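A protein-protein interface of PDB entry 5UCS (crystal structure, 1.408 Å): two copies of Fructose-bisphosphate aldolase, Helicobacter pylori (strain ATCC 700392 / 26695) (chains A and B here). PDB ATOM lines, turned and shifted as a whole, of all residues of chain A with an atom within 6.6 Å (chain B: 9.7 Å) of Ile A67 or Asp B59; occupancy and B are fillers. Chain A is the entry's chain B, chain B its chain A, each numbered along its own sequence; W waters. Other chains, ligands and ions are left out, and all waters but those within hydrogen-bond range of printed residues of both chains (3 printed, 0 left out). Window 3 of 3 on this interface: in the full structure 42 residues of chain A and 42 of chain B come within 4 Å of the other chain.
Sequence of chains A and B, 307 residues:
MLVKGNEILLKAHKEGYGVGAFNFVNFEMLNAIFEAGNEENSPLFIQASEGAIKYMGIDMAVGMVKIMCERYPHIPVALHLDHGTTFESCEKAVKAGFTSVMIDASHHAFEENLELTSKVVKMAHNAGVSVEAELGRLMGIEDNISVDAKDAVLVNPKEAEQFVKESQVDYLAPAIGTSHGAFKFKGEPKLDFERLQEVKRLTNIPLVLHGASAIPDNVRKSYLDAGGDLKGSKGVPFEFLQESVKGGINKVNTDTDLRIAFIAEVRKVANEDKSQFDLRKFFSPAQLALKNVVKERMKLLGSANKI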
ATOM      1  N   PHE A  34     -39.261  19.724  -1.384  1.00  0.00           N
ATOM      2  CA  PHE A  34     -38.186  18.739  -1.497  1.00  0.00           C
ATOM      3  C   PHE A  34     -38.464  17.490  -0.679  1.00  0.00           C
ATOM      4  O   PHE A  34     -38.246  16.370  -1.170  1.00  0.00           O
ATOM      5  CB  PHE A  34     -36.854  19.363  -1.102  1.00  0.00           C
ATOM      6  CG  PHE A  34     -36.070  19.885  -2.261  1.00  0.00           C
ATOM      7  CD1 PHE A  34     -36.317  21.148  -2.782  1.00  0.00           C
ATOM      8  CD2 PHE A  34     -35.068  19.120  -2.814  1.00  0.00           C
ATOM      9  CE1 PHE A  34     -35.604  21.610  -3.839  1.00  0.00           C
ATOM     10  CE2 PHE A  34     -34.355  19.580  -3.887  1.00  0.00           C
ATOM     11  CZ  PHE A  34     -34.598  20.843  -4.378  1.00  0.00           C
ATOM     12  N   VAL A  62     -31.907  30.886  -6.321  1.00  0.00           N
ATOM     13  CA  VAL A  62     -31.038  29.851  -6.871  1.00  0.00           C
ATOM     14  C   VAL A  62     -30.209  29.219  -5.768  1.00  0.00           C
ATOM     15  O   VAL A  62     -30.028  27.996  -5.722  1.00  0.00           O
ATOM     16  CB  VAL A  62     -30.158  30.396  -8.010  1.00  0.00           C
ATOM     17  CG1 VAL A  62     -29.287  29.303  -8.531  1.00  0.00           C
ATOM     18  CG2 VAL A  62     -30.995  30.928  -9.136  1.00  0.00           C
ATOM     19  N   GLY A  63     -29.691  30.047  -4.857  1.00  0.00           N
ATOM     20  CA  GLY A  63     -28.807  29.547  -3.823  1.00  0.00           C
ATOM     21  C   GLY A  63     -29.480  28.527  -2.922  1.00  0.00           C
ATOM     22  O   GLY A  63     -28.877  27.518  -2.554  1.00  0.00           O
ATOM     23  N   MET A  64     -30.713  28.804  -2.511  1.00  0.00           N
ATOM     24  CA  MET A  64     -31.419  27.860  -1.653  1.00  0.00           C
ATOM     25  C   MET A  64     -31.711  26.577  -2.413  1.00  0.00           C
ATOM     26  O   MET A  64     -31.613  25.478  -1.841  1.00  0.00           O
ATOM     27  CB  MET A  64     -32.723  28.467  -1.126  1.00  0.00           C
ATOM     28  CG  MET A  64     -32.521  29.514  -0.027  1.00  0.00           C
ATOM     29  SD  MET A  64     -34.046  29.920   0.839  1.00  0.00           S
ATOM     30  CE  MET A  64     -35.031  30.550  -0.500  1.00  0.00           C
ATOM     31  N   VAL A  65     -32.033  26.680  -3.710  1.00  0.00           N
ATOM     32  CA  VAL A  65     -32.288  25.457  -4.456  1.00  0.00           C
ATOM     33  C   VAL A  65     -31.019  24.616  -4.549  1.00  0.00           C
ATOM     34  O   VAL A  65     -31.057  23.382  -4.405  1.00  0.00           O
ATOM     35  CB  VAL A  65     -32.912  25.781  -5.825  1.00  0.00           C
ATOM     36  CG1 VAL A  65     -32.974  24.523  -6.691  1.00  0.00           C
ATOM     37  CG2 VAL A  65     -34.307  26.354  -5.632  1.00  0.00           C
ATOM     38  N   LYS A  66     -29.869  25.255  -4.777  1.00  0.00           N
ATOM     39  CA  LYS A  66     -28.631  24.488  -4.876  1.00  0.00           C
ATOM     40  C   LYS A  66     -28.304  23.777  -3.570  1.00  0.00           C
ATOM     41  O   LYS A  66     -27.882  22.615  -3.580  1.00  0.00           O
ATOM     42  CB  LYS A  66     -27.495  25.389  -5.328  1.00  0.00           C
ATOM     43  CG  LYS A  66     -27.610  25.831  -6.788  1.00  0.00           C
ATOM     44  CD  LYS A  66     -26.343  26.545  -7.242  1.00  0.00           C
ATOM     45  CE  LYS A  66     -26.433  27.044  -8.675  1.00  0.00           C
ATOM     46  NZ  LYS A  66     -26.744  25.963  -9.646  1.00  0.00           N
ATOM     47  N   ILE A  67     -28.530  24.433  -2.430  1.00  0.00           N
ATOM     48  CA  ILE A  67     -28.345  23.773  -1.142  1.00  0.00           C
ATOM     49  C   ILE A  67     -29.266  22.564  -1.029  1.00  0.00           C
ATOM     50  O   ILE A  67     -28.859  21.485  -0.571  1.00  0.00           O
ATOM     51  CB  ILE A  67     -28.578  24.771   0.006  1.00  0.00           C
ATOM     52  CG1 ILE A  67     -27.460  25.816  -0.014  1.00  0.00           C
ATOM     53  CG2 ILE A  67     -28.605  24.077   1.367  1.00  0.00           C
ATOM     54  CD1 ILE A  67     -27.784  27.091   0.719  1.00  0.00           C
ATOM     55  N   MET A  68     -30.526  22.722  -1.419  1.00  0.00           N
ATOM     56  CA  MET A  68     -31.470  21.617  -1.276  1.00  0.00           C
ATOM     57  C   MET A  68     -31.109  20.448  -2.192  1.00  0.00           C
ATOM     58  O   MET A  68     -31.247  19.282  -1.786  1.00  0.00           O
ATOM     59  CB  MET A  68     -32.905  22.111  -1.509  1.00  0.00           C
ATOM     60  CG  MET A  68     -33.386  23.116  -0.469  1.00  0.00           C
ATOM     61  SD  MET A  68     -33.440  22.455   1.226  1.00  0.00           S
ATOM     62  CE  MET A  68     -34.596  21.117   0.973  1.00  0.00           C
ATOM     63  N   CYS A  69     -30.670  20.745  -3.420  1.00  0.00           N
ATOM     64  CA  CYS A  69     -30.227  19.704  -4.347  1.00  0.00           C
ATOM     65  C   CYS A  69     -29.129  18.870  -3.717  1.00  0.00           C
ATOM     66  O   CYS A  69     -29.161  17.630  -3.765  1.00  0.00           O
ATOM     67  CB  CYS A  69     -29.736  20.347  -5.645  1.00  0.00           C
ATOM     68  SG  CYS A  69     -31.086  20.819  -6.685  1.00  0.00           S
ATOM     69  N   GLU A  70     -28.151  19.537  -3.104  1.00  0.00           N
ATOM     70  CA  GLU A  70     -27.027  18.830  -2.500  1.00  0.00           C
ATOM     71  C   GLU A  70     -27.508  17.965  -1.347  1.00  0.00           C
ATOM     72  O   GLU A  70     -26.944  16.896  -1.083  1.00  0.00           O
ATOM     73  CB  GLU A  70     -25.980  19.836  -2.005  1.00  0.00           C
ATOM     74  CG  GLU A  70     -25.234  20.562  -3.119  1.00  0.00           C
ATOM     75  CD  GLU A  70     -24.433  19.624  -4.012  1.00  0.00           C
ATOM     76  OE1 GLU A  70     -23.924  18.602  -3.505  1.00  0.00           O
ATOM     77  OE2 GLU A  70     -24.317  19.907  -5.223  1.00  0.00           O
ATOM     78  N   ARG A  71     -28.585  18.391  -0.686  1.00  0.00           N
ATOM     79  CA  ARG A  71     -29.162  17.602   0.395  1.00  0.00           C
ATOM     80  C   ARG A  71     -29.846  16.339  -0.123  1.00  0.00           C
ATOM     81  O   ARG A  71     -29.855  15.319   0.573  1.00  0.00           O
ATOM     82  CB  ARG A  71     -30.142  18.498   1.156  1.00  0.00           C
ATOM     83  CG  ARG A  71     -30.596  18.011   2.493  1.00  0.00           C
ATOM     84  CD  ARG A  71     -31.608  19.005   3.060  1.00  0.00           C
ATOM     85  NE  ARG A  71     -31.011  20.197   3.657  1.00  0.00           N
ATOM     86  CZ  ARG A  71     -31.717  21.064   4.377  1.00  0.00           C
ATOM     87  NH1 ARG A  71     -33.014  20.872   4.552  1.00  0.00           N
ATOM     88  NH2 ARG A  71     -31.120  22.112   4.942  1.00  0.00           N
ATOM     89  N   TYR A  72     -30.392  16.370  -1.344  1.00  0.00           N
ATOM     90  CA  TYR A  72     -31.114  15.241  -1.941  1.00  0.00           C
ATOM     91  C   TYR A  72     -30.573  14.977  -3.339  1.00  0.00           C
ATOM     92  O   TYR A  72     -31.281  15.149  -4.342  1.00  0.00           O
ATOM     93  CB  TYR A  72     -32.620  15.512  -1.992  1.00  0.00           C
ATOM     94  CG  TYR A  72     -33.274  15.748  -0.646  1.00  0.00           C
ATOM     95  CD1 TYR A  72     -33.542  17.031  -0.184  1.00  0.00           C
ATOM     96  CD2 TYR A  72     -33.643  14.690   0.152  1.00  0.00           C
ATOM     97  CE1 TYR A  72     -34.146  17.254   1.029  1.00  0.00           C
ATOM     98  CE2 TYR A  72     -34.252  14.894   1.378  1.00  0.00           C
ATOM     99  CZ  TYR A  72     -34.492  16.182   1.815  1.00  0.00           C
ATOM    100  OH  TYR A  72     -35.102  16.360   3.035  1.00  0.00           O
ATOM    101  N   PHE B  24     -32.043  34.215  13.979  1.00  0.00           N
ATOM    102  CA  PHE B  24     -32.905  33.918  12.836  1.00  0.00           C
ATOM    103  C   PHE B  24     -33.281  32.445  12.803  1.00  0.00           C
ATOM    104  O   PHE B  24     -32.516  31.588  13.263  1.00  0.00           O
ATOM    105  CB  PHE B  24     -32.271  34.332  11.505  1.00  0.00           C
ATOM    106  CG  PHE B  24     -31.197  33.405  10.982  1.00  0.00           C
ATOM    107  CD1 PHE B  24     -29.974  33.309  11.598  1.00  0.00           C
ATOM    108  CD2 PHE B  24     -31.417  32.655   9.838  1.00  0.00           C
ATOM    109  CE1 PHE B  24     -28.994  32.454  11.073  1.00  0.00           C
ATOM    110  CE2 PHE B  24     -30.444  31.858   9.316  1.00  0.00           C
ATOM    111  CZ  PHE B  24     -29.248  31.749   9.919  1.00  0.00           C
ATOM    112  N   LEU B  30     -33.656  36.615   8.524  1.00  0.00           N
ATOM    113  CA  LEU B  30     -32.295  36.930   8.095  1.00  0.00           C
ATOM    114  C   LEU B  30     -32.252  38.159   7.187  1.00  0.00           C
ATOM    115  O   LEU B  30     -31.368  39.022   7.319  1.00  0.00           O
ATOM    116  CB  LEU B  30     -31.683  35.715   7.398  1.00  0.00           C
ATOM    117  CG  LEU B  30     -30.201  35.805   7.065  1.00  0.00           C
ATOM    118  CD1 LEU B  30     -29.356  35.945   8.310  1.00  0.00           C
ATOM    119  CD2 LEU B  30     -29.787  34.598   6.249  1.00  0.00           C
ATOM    120  N   ALA B  52     -33.016  26.252  15.853  1.00  0.00           N
ATOM    121  CA  ALA B  52     -33.042  26.854  14.531  1.00  0.00           C
ATOM    122  C   ALA B  52     -32.218  26.055  13.540  1.00  0.00           C
ATOM    123  O   ALA B  52     -32.622  25.879  12.385  1.00  0.00           O
ATOM    124  CB  ALA B  52     -32.519  28.292  14.607  1.00  0.00           C
ATOM    125  N   ILE B  53     -31.064  25.547  13.970  1.00  0.00           N
ATOM    126  CA  ILE B  53     -30.237  24.710  13.107  1.00  0.00           C
ATOM    127  C   ILE B  53     -30.961  23.417  12.731  1.00  0.00           C
ATOM    128  O   ILE B  53     -30.902  22.957  11.577  1.00  0.00           O
ATOM    129  CB  ILE B  53     -28.882  24.444  13.793  1.00  0.00           C
ATOM    130  CG1 ILE B  53     -28.049  25.732  13.772  1.00  0.00           C
ATOM    131  CG2 ILE B  53     -28.127  23.280  13.100  1.00  0.00           C
ATOM    132  CD1 ILE B  53     -26.823  25.723  14.712  1.00  0.00           C
ATOM    133  N   LYS B  54     -31.670  22.796  13.681  1.00  0.00           N
ATOM    134  CA  LYS B  54     -32.413  21.594  13.332  1.00  0.00           C
ATOM    135  C   LYS B  54     -33.530  21.930  12.346  1.00  0.00           C
ATOM    136  O   LYS B  54     -33.790  21.166  11.410  1.00  0.00           O
ATOM    137  CB  LYS B  54     -32.970  20.955  14.603  1.00  0.00           C
ATOM    138  CG  LYS B  54     -33.643  19.595  14.366  1.00  0.00           C
ATOM    139  CD  LYS B  54     -34.051  18.922  15.671  1.00  0.00           C
ATOM    140  CE  LYS B  54     -32.845  18.567  16.547  1.00  0.00           C
ATOM    141  NZ  LYS B  54     -31.838  17.713  15.845  1.00  0.00           N
ATOM    142  N   TYR B  55     -34.169  23.085  12.534  1.00  0.00           N
ATOM    143  CA  TYR B  55     -35.292  23.500  11.694  1.00  0.00           C
ATOM    144  C   TYR B  55     -34.835  23.783  10.269  1.00  0.00           C
ATOM    145  O   TYR B  55     -35.468  23.325   9.309  1.00  0.00           O
ATOM    146  CB  TYR B  55     -35.939  24.743  12.313  1.00  0.00           C
ATOM    147  CG  TYR B  55     -37.088  25.370  11.550  1.00  0.00           C
ATOM    148  CD1 TYR B  55     -38.385  24.853  11.648  1.00  0.00           C
ATOM    149  CD2 TYR B  55     -36.893  26.470  10.741  1.00  0.00           C
ATOM    150  CE1 TYR B  55     -39.436  25.429  10.951  1.00  0.00           C
ATOM    151  CE2 TYR B  55     -37.953  27.059  10.043  1.00  0.00           C
ATOM    152  CZ  TYR B  55     -39.213  26.525  10.164  1.00  0.00           C
ATOM    153  OH  TYR B  55     -40.281  27.063   9.491  1.00  0.00           O
ATOM    154  N   MET B  56     -33.731  24.534  10.116  1.00  0.00           N
ATOM    155  CA  MET B  56     -33.229  24.922   8.798  1.00  0.00           C
ATOM    156  C   MET B  56     -32.361  23.850   8.161  1.00  0.00           C
ATOM    157  O   MET B  56     -32.324  23.738   6.923  1.00  0.00           O
ATOM    158  CB  MET B  56     -32.389  26.187   8.902  1.00  0.00           C
ATOM    159  CG  MET B  56     -33.193  27.456   8.938  1.00  0.00           C
ATOM    160  SD  MET B  56     -32.147  28.931   9.062  1.00  0.00           S
ATOM    161  CE  MET B  56     -31.694  28.879  10.796  1.00  0.00           C
ATOM    162  N   GLY B  57     -31.664  23.069   8.986  1.00  0.00           N
ATOM    163  CA  GLY B  57     -30.492  22.329   8.545  1.00  0.00           C
ATOM    164  C   GLY B  57     -29.267  23.222   8.585  1.00  0.00           C
ATOM    165  O   GLY B  57     -29.327  24.356   8.115  1.00  0.00           O
ATOM    166  N   ILE B  58     -28.157  22.750   9.147  1.00  0.00           N
ATOM    167  CA  ILE B  58     -26.988  23.621   9.287  1.00  0.00           C
ATOM    168  C   ILE B  58     -26.443  24.072   7.930  1.00  0.00           C
ATOM    169  O   ILE B  58     -25.893  25.181   7.811  1.00  0.00           O
ATOM    170  CB  ILE B  58     -25.907  22.976  10.176  1.00  0.00           C
ATOM    171  CG1 ILE B  58     -25.006  24.060  10.758  1.00  0.00           C
ATOM    172  CG2 ILE B  58     -25.127  21.916   9.406  1.00  0.00           C
ATOM    173  CD1 ILE B  58     -24.138  23.560  11.909  1.00  0.00           C
ATOM    174  N   ASP B  59     -26.603  23.240   6.890  1.00  0.00           N
ATOM    175  CA  ASP B  59     -26.181  23.601   5.540  1.00  0.00           C
ATOM    176  C   ASP B  59     -26.943  24.807   5.015  1.00  0.00           C
ATOM    177  O   ASP B  59     -26.367  25.670   4.343  1.00  0.00           O
ATOM    178  CB  ASP B  59     -26.350  22.399   4.600  1.00  0.00           C
ATOM    179  CG  ASP B  59     -27.766  21.765   4.627  1.00  0.00           C
ATOM    180  OD1 ASP B  59     -28.187  21.215   3.586  1.00  0.00           O
ATOM    181  OD2 ASP B  59     -28.466  21.742   5.664  1.00  0.00           O
ATOM    182  N   MET B  60     -28.239  24.880   5.313  1.00  0.00           N
ATOM    183  CA  MET B  60     -29.045  26.014   4.864  1.00  0.00           C
ATOM    184  C   MET B  60     -28.800  27.238   5.731  1.00  0.00           C
ATOM    185  O   MET B  60     -28.796  28.361   5.225  1.00  0.00           O
ATOM    186  CB  MET B  60     -30.521  25.653   4.912  1.00  0.00           C
ATOM    187  CG  MET B  60     -31.446  26.720   4.402  1.00  0.00           C
ATOM    188  SD  MET B  60     -31.226  27.077   2.637  1.00  0.00           S
ATOM    189  CE  MET B  60     -31.898  25.606   1.857  1.00  0.00           C
ATOM    190  N   ALA B  61     -28.604  27.049   7.037  1.00  0.00           N
ATOM    191  CA  ALA B  61     -28.330  28.189   7.907  1.00  0.00           C
ATOM    192  C   ALA B  61     -27.057  28.892   7.453  1.00  0.00           C
ATOM    193  O   ALA B  61     -27.053  30.110   7.210  1.00  0.00           O
ATOM    194  CB  ALA B  61     -28.210  27.737   9.357  1.00  0.00           C
ATOM    195  N   VAL B  62     -25.967  28.134   7.284  1.00  0.00           N
ATOM    196  CA  VAL B  62     -24.728  28.758   6.826  1.00  0.00           C
ATOM    197  C   VAL B  62     -24.886  29.260   5.398  1.00  0.00           C
ATOM    198  O   VAL B  62     -24.428  30.359   5.043  1.00  0.00           O
ATOM    199  CB  VAL B  62     -23.553  27.772   6.938  1.00  0.00           C
ATOM    200  CG1 VAL B  62     -22.283  28.392   6.381  1.00  0.00           C
ATOM    201  CG2 VAL B  62     -23.343  27.342   8.392  1.00  0.00           C
ATOM    202  N   GLY B  63     -25.512  28.444   4.541  1.00  0.00           N
ATOM    203  CA  GLY B  63     -25.598  28.799   3.134  1.00  0.00           C
ATOM    204  C   GLY B  63     -26.365  30.084   2.892  1.00  0.00           C
ATOM    205  O   GLY B  63     -25.934  30.932   2.101  1.00  0.00           O
ATOM    206  N   MET B  64     -27.493  30.272   3.585  1.00  0.00           N
ATOM    207  CA  MET B  64     -28.218  31.536   3.440  1.00  0.00           C
ATOM    208  C   MET B  64     -27.394  32.715   3.945  1.00  0.00           C
ATOM    209  O   MET B  64     -27.418  33.799   3.350  1.00  0.00           O
ATOM    210  CB  MET B  64     -29.584  31.508   4.141  1.00  0.00           C
ATOM    211  CG  MET B  64     -30.614  30.588   3.505  1.00  0.00           C
ATOM    212  SD  MET B  64     -32.282  30.813   4.159  1.00  0.00           S
ATOM    213  CE  MET B  64     -32.014  30.604   5.910  1.00  0.00           C
ATOM    214  N   VAL B  65     -26.697  32.547   5.071  1.00  0.00           N
ATOM    215  CA  VAL B  65     -25.881  33.655   5.561  1.00  0.00           C
ATOM    216  C   VAL B  65     -24.800  34.021   4.547  1.00  0.00           C
ATOM    217  O   VAL B  65     -24.521  35.208   4.314  1.00  0.00           O
ATOM    218  CB  VAL B  65     -25.297  33.324   6.943  1.00  0.00           C
ATOM    219  CG1 VAL B  65     -24.317  34.370   7.361  1.00  0.00           C
ATOM    220  CG2 VAL B  65     -26.409  33.239   7.947  1.00  0.00           C
ATOM    221  N   LYS B  66     -24.161  33.020   3.945  1.00  0.00           N
ATOM    222  CA  LYS B  66     -23.109  33.302   2.973  1.00  0.00           C
ATOM    223  C   LYS B  66     -23.664  34.045   1.761  1.00  0.00           C
ATOM    224  O   LYS B  66     -22.998  34.930   1.211  1.00  0.00           O
ATOM    225  CB  LYS B  66     -22.394  32.012   2.570  1.00  0.00           C
ATOM    226  CG  LYS B  66     -21.465  31.471   3.646  1.00  0.00           C
ATOM    227  CD  LYS B  66     -20.772  30.203   3.180  1.00  0.00           C
ATOM    228  CE  LYS B  66     -19.744  29.718   4.194  1.00  0.00           C
ATOM    229  NZ  LYS B  66     -19.144  28.412   3.793  1.00  0.00           N
ATOM    230  N   ILE B  67     -24.882  33.711   1.332  1.00  0.00           N
ATOM    231  CA  ILE B  67     -25.512  34.437   0.240  1.00  0.00           C
ATOM    232  C   ILE B  67     -25.736  35.888   0.636  1.00  0.00           C
ATOM    233  O   ILE B  67     -25.466  36.822  -0.138  1.00  0.00           O
ATOM    234  CB  ILE B  67     -26.824  33.745  -0.170  1.00  0.00           C
ATOM    235  CG1 ILE B  67     -26.490  32.417  -0.839  1.00  0.00           C
ATOM    236  CG2 ILE B  67     -27.602  34.600  -1.146  1.00  0.00           C
ATOM    237  CD1 ILE B  67     -27.625  31.457  -0.880  1.00  0.00           C
ATOM    238  N   MET B  68     -26.227  36.102   1.858  1.00  0.00           N
ATOM    239  CA  MET B  68     -26.486  37.464   2.321  1.00  0.00           C
ATOM    240  C   MET B  68     -25.190  38.261   2.467  1.00  0.00           C
ATOM    241  O   MET B  68     -25.165  39.459   2.159  1.00  0.00           O
ATOM    242  CB  MET B  68     -27.282  37.437   3.634  1.00  0.00           C
ATOM    243  CG  MET B  68     -28.691  36.827   3.483  1.00  0.00           C
ATOM    244  SD  MET B  68     -29.775  37.693   2.294  1.00  0.00           S
ATOM    245  CE  MET B  68     -29.796  39.310   3.032  1.00  0.00           C
ATOM    246  N   LEU B  79     -21.257  34.744  12.394  1.00  0.00           N
ATOM    247  CA  LEU B  79     -22.316  33.750  12.444  1.00  0.00           C
ATOM    248  C   LEU B  79     -22.068  32.874  13.660  1.00  0.00           C
ATOM    249  O   LEU B  79     -21.027  32.210  13.748  1.00  0.00           O
ATOM    250  CB  LEU B  79     -22.346  32.895  11.174  1.00  0.00           C
ATOM    251  CG  LEU B  79     -23.352  31.748  11.168  1.00  0.00           C
ATOM    252  CD1 LEU B  79     -24.758  32.213  11.496  1.00  0.00           C
ATOM    253  CD2 LEU B  79     -23.334  31.048   9.835  1.00  0.00           C
ATOM    254  N   LYS B  92     -19.705  20.611  15.193  1.00  0.00           N
ATOM    255  CA  LYS B  92     -20.448  20.604  13.935  1.00  0.00           C
ATOM    256  C   LYS B  92     -20.613  22.017  13.384  1.00  0.00           C
ATOM    257  O   LYS B  92     -20.558  22.226  12.165  1.00  0.00           O
ATOM    258  CB  LYS B  92     -21.816  19.964  14.133  1.00  0.00           C
ATOM    259  CG  LYS B  92     -21.765  18.432  14.124  1.00  0.00           C
ATOM    260  CD  LYS B  92     -23.118  17.793  14.365  1.00  0.00           C
ATOM    261  CE  LYS B  92     -23.032  16.279  14.107  1.00  0.00           C
ATOM    262  NZ  LYS B  92     -24.317  15.550  14.433  1.00  0.00           N
ATOM    263  N   ALA B  93     -20.839  23.002  14.263  1.00  0.00           N
ATOM    264  CA  ALA B  93     -20.997  24.377  13.799  1.00  0.00           C
ATOM    265  C   ALA B  93     -19.686  24.921  13.243  1.00  0.00           C
ATOM    266  O   ALA B  93     -19.675  25.539  12.173  1.00  0.00           O
ATOM    267  CB  ALA B  93     -21.512  25.273  14.928  1.00  0.00           C
ATOM    268  N   LYS B  95     -17.289  23.124  11.868  1.00  0.00           N
ATOM    269  CA  LYS B  95     -17.034  22.450  10.594  1.00  0.00           C
ATOM    270  C   LYS B  95     -17.929  22.974   9.480  1.00  0.00           C
ATOM    271  O   LYS B  95     -17.513  23.006   8.314  1.00  0.00           O
ATOM    272  CB  LYS B  95     -17.211  20.938  10.741  1.00  0.00           C
ATOM    273  CG  LYS B  95     -16.092  20.288  11.549  1.00  0.00           C
ATOM    274  CD  LYS B  95     -16.305  18.776  11.630  1.00  0.00           C
ATOM    275  CE  LYS B  95     -15.314  18.109  12.585  1.00  0.00           C
ATOM    276  NZ  LYS B  95     -15.629  16.662  12.821  1.00  0.00           N
ATOM    277  N   ALA B  96     -19.153  23.390   9.817  1.00  0.00           N
ATOM    278  CA  ALA B  96     -20.086  23.924   8.832  1.00  0.00           C
ATOM    279  C   ALA B  96     -19.773  25.362   8.438  1.00  0.00           C
ATOM    280  O   ALA B  96     -20.296  25.836   7.420  1.00  0.00           O
ATOM    281  CB  ALA B  96     -21.510  23.859   9.381  1.00  0.00           C
ATOM    282  N   GLY B  97     -18.973  26.075   9.219  1.00  0.00           N
ATOM    283  CA  GLY B  97     -18.564  27.409   8.833  1.00  0.00           C
ATOM    284  C   GLY B  97     -19.025  28.537   9.735  1.00  0.00           C
ATOM    285  O   GLY B  97     -18.885  29.708   9.368  1.00  0.00           O
ATOM    286  N   PHE B  98     -19.554  28.230  10.916  1.00  0.00           N
ATOM    287  CA  PHE B  98     -19.798  29.285  11.893  1.00  0.00           C
ATOM    288  C   PHE B  98     -18.475  29.926  12.291  1.00  0.00           C
ATOM    289  O   PHE B  98     -17.420  29.283  12.297  1.00  0.00           O
ATOM    290  CB  PHE B  98     -20.494  28.708  13.132  1.00  0.00           C
ATOM    291  CG  PHE B  98     -21.982  28.485  12.965  1.00  0.00           C
ATOM    292  CD1 PHE B  98     -22.484  27.582  12.035  1.00  0.00           C
ATOM    293  CD2 PHE B  98     -22.889  29.176  13.746  1.00  0.00           C
ATOM    294  CE1 PHE B  98     -23.847  27.394  11.917  1.00  0.00           C
ATOM    295  CE2 PHE B  98     -24.252  28.988  13.623  1.00  0.00           C
ATOM    296  CZ  PHE B  98     -24.732  28.101  12.717  1.00  0.00           C
HETATM  297  O   HOH W   1     -29.532  19.338   6.671  1.00  0.00           O
HETATM  298  O   HOH W   2     -26.858  20.951   1.284  1.00  0.00           O
HETATM  299  O   HOH W   3     -34.493  21.454   7.215  1.00  0.00           O
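Of the 12 printed residues of chain A, 5 touch a printed residue of chain B.
Hydrophobic or aromatic side chains of chain A that line the printed part of chain B: Met A64, Ile A67 and Met A68.
Among the printed residues, 11 pairs touch across the chains.
Among the printed residues, Asp or Glu carboxylates within 4 Å of a Lys or Arg side-chain nitrogen of the other chain: Arg A71 with Asp B59 (2.8 Å).
Among the printed residues, merely in contact across the chains: Gly A63 with Ile B67, Met A64 with Met B60, Met A64 with Met B64, Ile A67 with Asp B59, Ile A67 with Met B60, Ile A67 with Gly B63, Met A68 with Met B60, Arg A71 with Gly B57 and Arg A71 with Met B60.
Water W2 lies within hydrogen-bond range of the side-chain carboxylate of Asp B59 (2.7 Å) and the backbone carbonyl oxygen of Ile A67 (2.8 Å).
Water W1 lies within hydrogen-bond range of the side-chain carboxylate (OD2) of Asp B59 and the guanidinium group (NE) of Arg A71.
Water W3 lies within hydrogen-bond range of the backbone carbonyl oxygen (O) of Tyr B55, the guanidinium group (NH1) of Arg A71 and the backbone carbonyl oxygen (O) of Met B56.
Gly A63 touches Ile B67, and with the chains exchanged Ile A67 touches Gly B63.
Met A64 touches its own counterpart, Met B64.
Of the 11 pairs that touch across the chains among the printed residues, 3 have their exchanged pair printed and touching as well.
Asp B59 touches just these residues of chain A: Ile A67 and Arg A71.
Of the printed residues of chain A, Met B60 touches Met A64, Ile A67, Met A68 and Arg A71.
Printed residues of chain A within 4 Å of Gly B63: Ile A67 (3.7 Å).
Printed residues of chain A within 4 Å of Met B64: Met A64.
The nearest printed residue of chain A that does not touch Gly B63 is Gly A63 (6.5 Å).
The side-chain sulfur (SD) of Met A68 lies within hydrogen-bond range of the guanidinium group (NH1) of Arg A71 (3.7 Å).
The side-chain carboxylate of Asp B59 lies within salt-bridge range of the guanidinium group of Arg A71.
The backbone carbonyl oxygen (O) of Met B56 lies within hydrogen-bond range of the guanidinium group (NH2) of Arg A71, at 2.8 Å.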
